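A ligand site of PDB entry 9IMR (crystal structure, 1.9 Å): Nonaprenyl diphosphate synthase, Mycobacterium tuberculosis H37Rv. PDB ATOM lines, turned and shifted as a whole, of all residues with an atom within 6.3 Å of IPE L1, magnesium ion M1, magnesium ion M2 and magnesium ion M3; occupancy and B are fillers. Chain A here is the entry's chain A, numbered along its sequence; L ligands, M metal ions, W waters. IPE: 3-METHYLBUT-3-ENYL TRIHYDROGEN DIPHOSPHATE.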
ATOM      1  N   HIS A  90     -11.616 -20.052 -26.508  1.00  0.00           N
ATOM      2  CA  HIS A  90     -12.952 -20.519 -26.917  1.00  0.00           C
ATOM      3  C   HIS A  90     -12.773 -21.625 -27.939  1.00  0.00           C
ATOM      4  O   HIS A  90     -13.336 -22.702 -27.762  1.00  0.00           O
ATOM      5  CB  HIS A  90     -13.783 -19.359 -27.413  1.00  0.00           C
ATOM      6  CG  HIS A  90     -15.081 -19.781 -28.028  1.00  0.00           C
ATOM      7  ND1 HIS A  90     -16.060 -20.394 -27.302  1.00  0.00           N
ATOM      8  CD2 HIS A  90     -15.545 -19.652 -29.297  1.00  0.00           C
ATOM      9  CE1 HIS A  90     -17.100 -20.644 -28.069  1.00  0.00           C
ATOM     10  NE2 HIS A  90     -16.826 -20.146 -29.310  1.00  0.00           N
ATOM     11  N   THR A  93     -11.595 -24.930 -26.501  1.00  0.00           N
ATOM     12  CA  THR A  93     -12.690 -25.618 -25.774  1.00  0.00           C
ATOM     13  C   THR A  93     -13.609 -26.327 -26.775  1.00  0.00           C
ATOM     14  O   THR A  93     -14.127 -27.365 -26.406  1.00  0.00           O
ATOM     15  CB  THR A  93     -13.433 -24.683 -24.815  1.00  0.00           C
ATOM     16  OG1 THR A  93     -14.180 -23.710 -25.555  1.00  0.00           O
ATOM     17  CG2 THR A  93     -12.481 -24.036 -23.849  1.00  0.00           C
ATOM     18  N   LEU A  94     -13.856 -25.765 -27.974  1.00  0.00           N
ATOM     19  CA  LEU A  94     -14.788 -26.410 -28.951  1.00  0.00           C
ATOM     20  C   LEU A  94     -14.181 -27.739 -29.409  1.00  0.00           C
ATOM     21  O   LEU A  94     -14.923 -28.711 -29.554  1.00  0.00           O
ATOM     22  CB  LEU A  94     -15.095 -25.521 -30.154  1.00  0.00           C
ATOM     23  CG  LEU A  94     -15.728 -24.165 -29.872  1.00  0.00           C
ATOM     24  CD1 LEU A  94     -16.153 -23.500 -31.181  1.00  0.00           C
ATOM     25  CD2 LEU A  94     -16.907 -24.284 -28.952  1.00  0.00           C
ATOM     26  N   ASP A  97     -14.664 -30.080 -26.517  1.00  0.00           N
ATOM     27  CA  ASP A  97     -16.078 -30.266 -26.198  1.00  0.00           C
ATOM     28  C   ASP A  97     -16.721 -31.193 -27.267  1.00  0.00           C
ATOM     29  O   ASP A  97     -17.497 -32.084 -26.901  1.00  0.00           O
ATOM     30  CB  ASP A  97     -16.789 -28.921 -26.069  1.00  0.00           C
ATOM     31  CG  ASP A  97     -18.253 -29.147 -25.752  1.00  0.00           C
ATOM     32  OD1 ASP A  97     -18.567 -29.389 -24.550  1.00  0.00           O
ATOM     33  OD2 ASP A  97     -19.069 -29.214 -26.720  1.00  0.00           O
ATOM     34  N   ASP A  98     -16.349 -31.019 -28.526  1.00  0.00           N
ATOM     35  CA  ASP A  98     -16.901 -31.852 -29.630  1.00  0.00           C
ATOM     36  C   ASP A  98     -16.473 -33.309 -29.477  1.00  0.00           C
ATOM     37  O   ASP A  98     -17.290 -34.231 -29.734  1.00  0.00           O
ATOM     38  CB  ASP A  98     -16.563 -31.231 -30.981  1.00  0.00           C
ATOM     39  CG  ASP A  98     -17.510 -30.103 -31.387  1.00  0.00           C
ATOM     40  OD1 ASP A  98     -18.549 -29.940 -30.763  1.00  0.00           O
ATOM     41  OD2 ASP A  98     -17.113 -29.354 -32.300  1.00  0.00           O
ATOM     42  N   MET A 100     -15.819 -34.760 -26.505  1.00  0.00           N
ATOM     43  CA  MET A 100     -16.552 -35.216 -25.282  1.00  0.00           C
ATOM     44  C   MET A 100     -18.026 -35.402 -25.579  1.00  0.00           C
ATOM     45  O   MET A 100     -18.590 -36.366 -25.062  1.00  0.00           O
ATOM     46  CB  MET A 100     -16.369 -34.234 -24.111  1.00  0.00           C
ATOM     47  CG  MET A 100     -14.889 -34.194 -23.666  1.00  0.00           C
ATOM     48  SD  MET A 100     -14.710 -33.275 -22.136  1.00  0.00           S
ATOM     49  CE  MET A 100     -15.317 -31.651 -22.607  1.00  0.00           C
ATOM     50  N   ASP A 101     -18.625 -34.554 -26.406  1.00  0.00           N
ATOM     51  CA  ASP A 101     -20.061 -34.618 -26.725  1.00  0.00           C
ATOM     52  C   ASP A 101     -20.302 -35.489 -27.961  1.00  0.00           C
ATOM     53  O   ASP A 101     -21.462 -35.568 -28.405  1.00  0.00           O
ATOM     54  CB  ASP A 101     -20.621 -33.201 -26.825  1.00  0.00           C
ATOM     55  CG  ASP A 101     -20.601 -32.466 -25.502  1.00  0.00           C
ATOM     56  OD1 ASP A 101     -20.483 -33.128 -24.444  1.00  0.00           O
ATOM     57  OD2 ASP A 101     -20.709 -31.228 -25.522  1.00  0.00           O
ATOM     58  N   ALA A 103     -19.815 -34.942 -30.997  1.00  0.00           N
ATOM     59  CA  ALA A 103     -20.503 -34.096 -31.988  1.00  0.00           C
ATOM     60  C   ALA A 103     -19.893 -34.392 -33.351  1.00  0.00           C
ATOM     61  O   ALA A 103     -18.653 -34.508 -33.457  1.00  0.00           O
ATOM     62  CB  ALA A 103     -20.338 -32.648 -31.589  1.00  0.00           C
ATOM     63  N   ARG A 106     -19.998 -29.072 -36.450  1.00  0.00           N
ATOM     64  CA  ARG A 106     -19.718 -27.778 -35.769  1.00  0.00           C
ATOM     65  C   ARG A 106     -19.605 -26.684 -36.814  1.00  0.00           C
ATOM     66  O   ARG A 106     -18.913 -26.889 -37.793  1.00  0.00           O
ATOM     67  CB  ARG A 106     -18.402 -27.916 -35.019  1.00  0.00           C
ATOM     68  CG  ARG A 106     -17.833 -26.625 -34.438  1.00  0.00           C
ATOM     69  CD  ARG A 106     -18.618 -26.100 -33.253  1.00  0.00           C
ATOM     70  NE  ARG A 106     -18.425 -26.877 -32.013  1.00  0.00           N
ATOM     71  CZ  ARG A 106     -19.104 -26.637 -30.896  1.00  0.00           C
ATOM     72  NH1 ARG A 106     -19.929 -25.606 -30.828  1.00  0.00           N
ATOM     73  NH2 ARG A 106     -18.985 -27.419 -29.838  1.00  0.00           N
ATOM     74  N   LEU A 154     -13.303 -22.707 -16.350  1.00  0.00           N
ATOM     75  CA  LEU A 154     -14.067 -23.244 -17.510  1.00  0.00           C
ATOM     76  C   LEU A 154     -13.962 -24.764 -17.490  1.00  0.00           C
ATOM     77  O   LEU A 154     -15.000 -25.425 -17.593  1.00  0.00           O
ATOM     78  CB  LEU A 154     -13.398 -22.645 -18.750  1.00  0.00           C
ATOM     79  CG  LEU A 154     -14.043 -22.898 -20.072  1.00  0.00           C
ATOM     80  CD1 LEU A 154     -13.459 -21.897 -21.104  1.00  0.00           C
ATOM     81  CD2 LEU A 154     -13.798 -24.333 -20.494  1.00  0.00           C
ATOM     82  N   GLN A 158     -16.839 -27.716 -17.017  1.00  0.00           N
ATOM     83  CA  GLN A 158     -16.970 -28.882 -17.931  1.00  0.00           C
ATOM     84  C   GLN A 158     -16.930 -30.175 -17.111  1.00  0.00           C
ATOM     85  O   GLN A 158     -17.708 -31.093 -17.391  1.00  0.00           O
ATOM     86  CB  GLN A 158     -15.885 -28.877 -19.003  1.00  0.00           C
ATOM     87  CG  GLN A 158     -16.042 -27.759 -20.044  1.00  0.00           C
ATOM     88  CD  GLN A 158     -17.047 -28.088 -21.123  1.00  0.00           C
ATOM     89  OE1 GLN A 158     -16.695 -28.385 -22.287  1.00  0.00           O
ATOM     90  NE2 GLN A 158     -18.294 -28.054 -20.747  1.00  0.00           N
ATOM     91  N   GLU A 161     -20.061 -30.623 -15.015  1.00  0.00           N
ATOM     92  CA  GLU A 161     -21.175 -31.089 -15.866  1.00  0.00           C
ATOM     93  C   GLU A 161     -21.050 -32.602 -16.060  1.00  0.00           C
ATOM     94  O   GLU A 161     -22.078 -33.318 -15.940  1.00  0.00           O
ATOM     95  CB  GLU A 161     -21.102 -30.408 -17.209  1.00  0.00           C
ATOM     96  CG  GLU A 161     -22.265 -30.767 -18.091  1.00  0.00           C
ATOM     97  CD  GLU A 161     -22.188 -30.017 -19.397  1.00  0.00           C
ATOM     98  OE1 GLU A 161     -21.688 -30.595 -20.342  1.00  0.00           O
ATOM     99  OE2 GLU A 161     -22.655 -28.872 -19.453  1.00  0.00           O
ATOM    100  N   LYS A 182     -18.529 -22.919 -16.950  1.00  0.00           N
ATOM    101  CA  LYS A 182     -18.085 -23.405 -18.300  1.00  0.00           C
ATOM    102  C   LYS A 182     -18.273 -22.313 -19.372  1.00  0.00           C
ATOM    103  O   LYS A 182     -17.557 -22.373 -20.341  1.00  0.00           O
ATOM    104  CB  LYS A 182     -18.748 -24.720 -18.731  1.00  0.00           C
ATOM    105  CG  LYS A 182     -20.239 -24.666 -19.008  1.00  0.00           C
ATOM    106  CD  LYS A 182     -20.725 -25.875 -19.800  1.00  0.00           C
ATOM    107  CE  LYS A 182     -22.149 -25.673 -20.241  1.00  0.00           C
ATOM    108  NZ  LYS A 182     -22.676 -26.786 -21.061  1.00  0.00           N
ATOM    109  N   THR A 183     -19.163 -21.340 -19.165  1.00  0.00           N
ATOM    110  CA  THR A 183     -19.527 -20.337 -20.198  1.00  0.00           C
ATOM    111  C   THR A 183     -19.369 -18.918 -19.655  1.00  0.00           C
ATOM    112  O   THR A 183     -18.932 -18.027 -20.403  1.00  0.00           O
ATOM    113  CB  THR A 183     -20.925 -20.646 -20.733  1.00  0.00           C
ATOM    114  OG1 THR A 183     -20.965 -22.022 -21.173  1.00  0.00           O
ATOM    115  CG2 THR A 183     -21.310 -19.740 -21.890  1.00  0.00           C
ATOM    116  N   GLN A 220     -25.563 -19.488 -22.263  1.00  0.00           N
ATOM    117  CA  GLN A 220     -25.562 -20.974 -22.156  1.00  0.00           C
ATOM    118  C   GLN A 220     -27.025 -21.473 -22.071  1.00  0.00           C
ATOM    119  O   GLN A 220     -27.354 -22.529 -22.627  1.00  0.00           O
ATOM    120  CB  GLN A 220     -24.805 -21.529 -20.942  1.00  0.00           C
ATOM    121  CG  GLN A 220     -24.711 -23.047 -21.055  1.00  0.00           C
ATOM    122  CD  GLN A 220     -24.050 -23.538 -22.317  1.00  0.00           C
ATOM    123  OE1 GLN A 220     -24.525 -24.495 -22.984  1.00  0.00           O
ATOM    124  NE2 GLN A 220     -22.891 -22.975 -22.612  1.00  0.00           N
ATOM    125  N   ASP A 223     -28.148 -21.436 -25.486  1.00  0.00           N
ATOM    126  CA  ASP A 223     -27.472 -22.531 -26.202  1.00  0.00           C
ATOM    127  C   ASP A 223     -28.267 -23.834 -25.934  1.00  0.00           C
ATOM    128  O   ASP A 223     -28.430 -24.620 -26.894  1.00  0.00           O
ATOM    129  CB  ASP A 223     -26.030 -22.720 -25.753  1.00  0.00           C
ATOM    130  CG  ASP A 223     -25.398 -23.803 -26.577  1.00  0.00           C
ATOM    131  OD1 ASP A 223     -25.204 -23.566 -27.800  1.00  0.00           O
ATOM    132  OD2 ASP A 223     -25.131 -24.874 -26.030  1.00  0.00           O
ATOM    133  N   ASP A 224     -28.739 -24.012 -24.708  1.00  0.00           N
ATOM    134  CA  ASP A 224     -29.450 -25.239 -24.274  1.00  0.00           C
ATOM    135  C   ASP A 224     -30.834 -25.273 -24.936  1.00  0.00           C
ATOM    136  O   ASP A 224     -31.287 -26.336 -25.286  1.00  0.00           O
ATOM    137  CB  ASP A 224     -29.502 -25.288 -22.763  1.00  0.00           C
ATOM    138  CG  ASP A 224     -28.144 -25.461 -22.117  1.00  0.00           C
ATOM    139  OD1 ASP A 224     -27.188 -25.743 -22.821  1.00  0.00           O
ATOM    140  OD2 ASP A 224     -28.079 -25.279 -20.913  1.00  0.00           O
ATOM    141  N   ASP A 227     -30.382 -26.069 -28.570  1.00  0.00           N
ATOM    142  CA  ASP A 227     -30.109 -27.512 -28.765  1.00  0.00           C
ATOM    143  C   ASP A 227     -31.433 -28.254 -29.000  1.00  0.00           C
ATOM    144  O   ASP A 227     -31.412 -29.311 -29.677  1.00  0.00           O
ATOM    145  CB  ASP A 227     -29.395 -28.107 -27.571  1.00  0.00           C
ATOM    146  CG  ASP A 227     -28.504 -29.276 -27.924  1.00  0.00           C
ATOM    147  OD1 ASP A 227     -27.409 -28.991 -28.439  1.00  0.00           O
ATOM    148  OD2 ASP A 227     -28.884 -30.457 -27.653  1.00  0.00           O
ATOM    149  N   LYS A 237     -25.050 -26.943 -36.041  1.00  0.00           N
ATOM    150  CA  LYS A 237     -24.793 -28.200 -35.317  1.00  0.00           C
ATOM    151  C   LYS A 237     -26.097 -28.978 -35.218  1.00  0.00           C
ATOM    152  O   LYS A 237     -27.130 -28.463 -35.605  1.00  0.00           O
ATOM    153  CB  LYS A 237     -24.162 -27.925 -33.961  1.00  0.00           C
ATOM    154  CG  LYS A 237     -24.838 -26.870 -33.137  1.00  0.00           C
ATOM    155  CD  LYS A 237     -23.990 -26.401 -31.948  1.00  0.00           C
ATOM    156  CE  LYS A 237     -24.899 -25.625 -31.042  1.00  0.00           C
ATOM    157  NZ  LYS A 237     -24.235 -25.093 -29.839  1.00  0.00           N
ATOM    158  N   THR A 241     -28.190 -33.037 -29.281  1.00  0.00           N
ATOM    159  CA  THR A 241     -26.906 -33.480 -28.691  1.00  0.00           C
ATOM    160  C   THR A 241     -27.009 -33.673 -27.177  1.00  0.00           C
ATOM    161  O   THR A 241     -26.460 -34.683 -26.686  1.00  0.00           O
ATOM    162  CB  THR A 241     -25.785 -32.527 -29.133  1.00  0.00           C
ATOM    163  OG1 THR A 241     -25.720 -32.573 -30.564  1.00  0.00           O
ATOM    164  CG2 THR A 241     -24.448 -32.937 -28.551  1.00  0.00           C
ATOM    165  N   ASP A 242     -27.650 -32.781 -26.435  1.00  0.00           N
ATOM    166  CA  ASP A 242     -27.711 -32.891 -24.949  1.00  0.00           C
ATOM    167  C   ASP A 242     -28.513 -34.149 -24.589  1.00  0.00           C
ATOM    168  O   ASP A 242     -28.097 -34.935 -23.673  1.00  0.00           O
ATOM    169  CB  ASP A 242     -28.271 -31.613 -24.328  1.00  0.00           C
ATOM    170  CG  ASP A 242     -27.425 -30.391 -24.618  1.00  0.00           C
ATOM    171  OD1 ASP A 242     -26.205 -30.519 -24.670  1.00  0.00           O
ATOM    172  OD2 ASP A 242     -28.024 -29.298 -24.677  1.00  0.00           O
ATOM    173  N   VAL A 247     -26.937 -35.020 -21.099  1.00  0.00           N
ATOM    174  CA  VAL A 247     -26.666 -33.796 -20.302  1.00  0.00           C
ATOM    175  C   VAL A 247     -28.031 -33.149 -20.022  1.00  0.00           C
ATOM    176  O   VAL A 247     -28.673 -32.792 -21.005  1.00  0.00           O
ATOM    177  CB  VAL A 247     -25.736 -32.849 -21.077  1.00  0.00           C
ATOM    178  CG1 VAL A 247     -25.546 -31.522 -20.366  1.00  0.00           C
ATOM    179  CG2 VAL A 247     -24.393 -33.546 -21.368  1.00  0.00           C
HETATM  180  C1  IPE L   1     -20.508 -25.423 -23.877  1.00  0.00           C
HETATM  181  O1  IPE L   1     -21.589 -26.389 -23.736  1.00  0.00           O
HETATM  182  C2  IPE L   1     -19.206 -26.139 -23.901  1.00  0.00           C
HETATM  183  C3  IPE L   1     -17.984 -25.256 -24.061  1.00  0.00           C
HETATM  184  C4  IPE L   1     -17.282 -25.252 -25.180  1.00  0.00           C
HETATM  185  C5  IPE L   1     -17.574 -24.457 -22.877  1.00  0.00           C
HETATM  186  PA  IPE L   1     -22.120 -27.224 -25.011  1.00  0.00           P
HETATM  187  O1A IPE L   1     -23.597 -27.262 -24.912  1.00  0.00           O
HETATM  188  O2A IPE L   1     -21.436 -28.560 -25.132  1.00  0.00           O
HETATM  189  O3A IPE L   1     -21.728 -26.356 -26.272  1.00  0.00           O
HETATM  190  PB  IPE L   1     -22.091 -26.773 -27.806  1.00  0.00           P
HETATM  191  O1B IPE L   1     -21.598 -25.617 -28.648  1.00  0.00           O
HETATM  192  O2B IPE L   1     -23.605 -26.904 -27.849  1.00  0.00           O
HETATM  193  O3B IPE L   1     -21.358 -28.068 -28.060  1.00  0.00           O
HETATM  194  C1  IPE L   2     -20.461 -22.680 -28.358  1.00  0.00           C
HETATM  195  O1  IPE L   2     -20.207 -21.247 -28.347  1.00  0.00           O
HETATM  196  C2  IPE L   2     -19.998 -23.191 -27.037  1.00  0.00           C
HETATM  197  C3  IPE L   2     -20.709 -22.571 -25.868  1.00  0.00           C
HETATM  198  C4  IPE L   2     -20.053 -21.997 -24.869  1.00  0.00           C
HETATM  199  C5  IPE L   2     -22.194 -22.704 -25.888  1.00  0.00           C
HETATM  200  PA  IPE L   2     -20.717 -20.361 -29.553  1.00  0.00           P
HETATM  201  O1A IPE L   2     -22.172 -20.597 -29.772  1.00  0.00           O
HETATM  202  O2A IPE L   2     -20.270 -18.938 -29.352  1.00  0.00           O
HETATM  203  O3A IPE L   2     -19.943 -20.975 -30.810  1.00  0.00           O
HETATM  204  PB  IPE L   2     -19.368 -20.330 -32.212  1.00  0.00           P
HETATM  205  O1B IPE L   2     -18.019 -19.775 -31.830  1.00  0.00           O
HETATM  206  O2B IPE L   2     -20.356 -19.265 -32.674  1.00  0.00           O
HETATM  207  O3B IPE L   2     -19.226 -21.515 -33.122  1.00  0.00           O
HETATM  208 MG    MG M   1     -20.453 -29.936 -23.805  1.00  0.00          MG
HETATM  209 MG    MG M   2     -20.926 -29.702 -26.994  1.00  0.00          MG
HETATM  210 MG    MG M   3     -25.021 -26.838 -26.403  1.00  0.00          MG
HETATM  211  O   HOH W   1     -25.309 -29.056 -26.720  1.00  0.00           O
HETATM  212  O   HOH W   2     -26.565 -27.085 -24.999  1.00  0.00           O
HETATM  213  O   HOH W   3     -19.474 -31.448 -22.606  1.00  0.00           O
HETATM  214  O   HOH W   4     -20.405 -28.812 -22.053  1.00  0.00           O
HETATM  215  O   HOH W   5     -22.361 -30.629 -22.997  1.00  0.00           O
HETATM  216  O   HOH W   6     -22.937 -30.342 -27.094  1.00  0.00           O
HETATM  217  O   HOH W   7     -24.603 -29.050 -23.095  1.00  0.00           O
HETATM  218  O   HOH W   8     -20.446 -30.689 -28.785  1.00  0.00           O
HETATM  219  O   HOH W   9     -24.546 -28.883 -29.655  1.00  0.00           O
HETATM  220  O   HOH W  10     -26.486 -26.553 -28.037  1.00  0.00           O
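The guanidinium group (NH1) of Arg 106 lies within salt-bridge range of an oxygen (O1B) of IPE L1, 2.7 Å away.
The side-chain amino group of Lys 237 lies within salt-bridge range of an oxygen (O1B) of IPE L1.
An oxygen (O1) of IPE L1 sits at hydrogen-bond distance from the side-chain amino group of Lys 182 (2.9 Å).
OE1 of Gln 220 lies close to O1A of IPE L1, 3.5 Å away.
O1B of IPE L2 sits at hydrogen-bond distance from NE2 of His 90 (2.8 Å).
The side-chain carboxylate of Asp 97 sits close to the side-chain amide oxygen of Gln 158 (3.1 Å).
The side-chain amino group (NZ) of Lys 237 lies within salt-bridge range of the side-chain carboxylate (OD1) of Asp 223, at 2.7 Å.
The side-chain carboxylate (OD2) of Asp 223 lies close to the side-chain amide oxygen (OE1) of Gln 220 (3.1 Å).
OD1 of Asp 98 lies within salt-bridge range of NH2 of Arg 106, 2.7 Å away.
OG1 of Thr 93 sits at hydrogen-bond distance from O of His 90.
OG1 of Thr 183 sits at hydrogen-bond distance from NE2 of Gln 220 (2.6 Å).
The side-chain carboxylate (OD2) of Asp 227 is in hydrogen-bond range of the backbone NH (N) of Asp 242 (2.9 Å).
The side-chain carboxylate (OD2) of Asp 227 sits at hydrogen-bond distance from the backbone NH (N) of Thr 241, at 3.1 Å.
Merely in contact with IPE L1: Thr 93 (3.5 Å), Gln 158 (3.7 Å) and Leu 94 (3.9 Å).
Of the 22 residues printed, 10 come within 4 Å of IPE L1.
The nearest printed residue that does not touch IPE L1 is Asp 242 (4.2 Å).
Merely in contact with magnesium ion M1: Glu 161 (3.7 Å).
Of the 22 residues printed, 2 come within 4 Å of magnesium ion M2.
The nearest printed residue that does not touch magnesium ion M2 is Arg 106 (4.1 Å).
Asp 227 touches magnesium ion M3.
Lys 237 touches magnesium ion M3 (NZ to MG, 3.9 Å).
Along chain A the residues within 4 Å of magnesium ion M3 span positions 223 to 237.
The nearest printed residue that does not touch magnesium ion M3 is Gln 220 (4.2 Å).
Magnesium ion M1 is bound by water W4, the side-chain carboxylate (OD1) of Asp 97, an oxygen (O2A) of IPE L1, the side-chain carboxylate (OD2) of Asp 101, water W3 and water W5.
Magnesium ion M1 has six donor atoms within binding distance.
Magnesium ion M2 is bound by the side-chain carboxylate (OD2) of Asp 97, an oxygen (O3B) of IPE L1, water W8, water W6, the side-chain carboxylate (OD2) of Asp 101 and an oxygen (O2A) of IPE L1.
Magnesium ion M3 is bound by the side-chain carboxylate (OD2) of Asp 223, an oxygen (O2B) of IPE L1, water W2, an oxygen (O1A) of IPE L1, water W10 and water W1.
Magnesium ion M3 has six donor atoms within binding distance.
Water W4 lies within hydrogen-bond range of the side-chain amide nitrogen of Gln 158 (2.6 Å), the side-chain carboxylate of Glu 161 (2.8 Å), an oxygen (O1) of IPE L1 (3.2 Å) and the side-chain amino group of Lys 182 (3.2 Å).
Water W3 lies within hydrogen-bond range of OD1 of Asp 101 (2.7 Å) and OE1 of Glu 161 (3.3 Å).
Water W5 lies within hydrogen-bond range of OE1 of Glu 161 (2.7 Å) and OD1 of Asp 101 (3.4 Å).
Water W2 bridges OD1 of Asp 224 and OD2 of Asp 242.
Water W1 lies within hydrogen-bond range of the side-chain carboxylate (OD1) of Asp 242 (2.7 Å) and the side-chain carboxylate (OD1) of Asp 227 (2.7 Å).
Water W10 lies within hydrogen-bond range of OD1 of Asp 227 (2.6 Å), O of Asp 223 (3.0 Å) and NZ of Lys 237 (3.2 Å).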
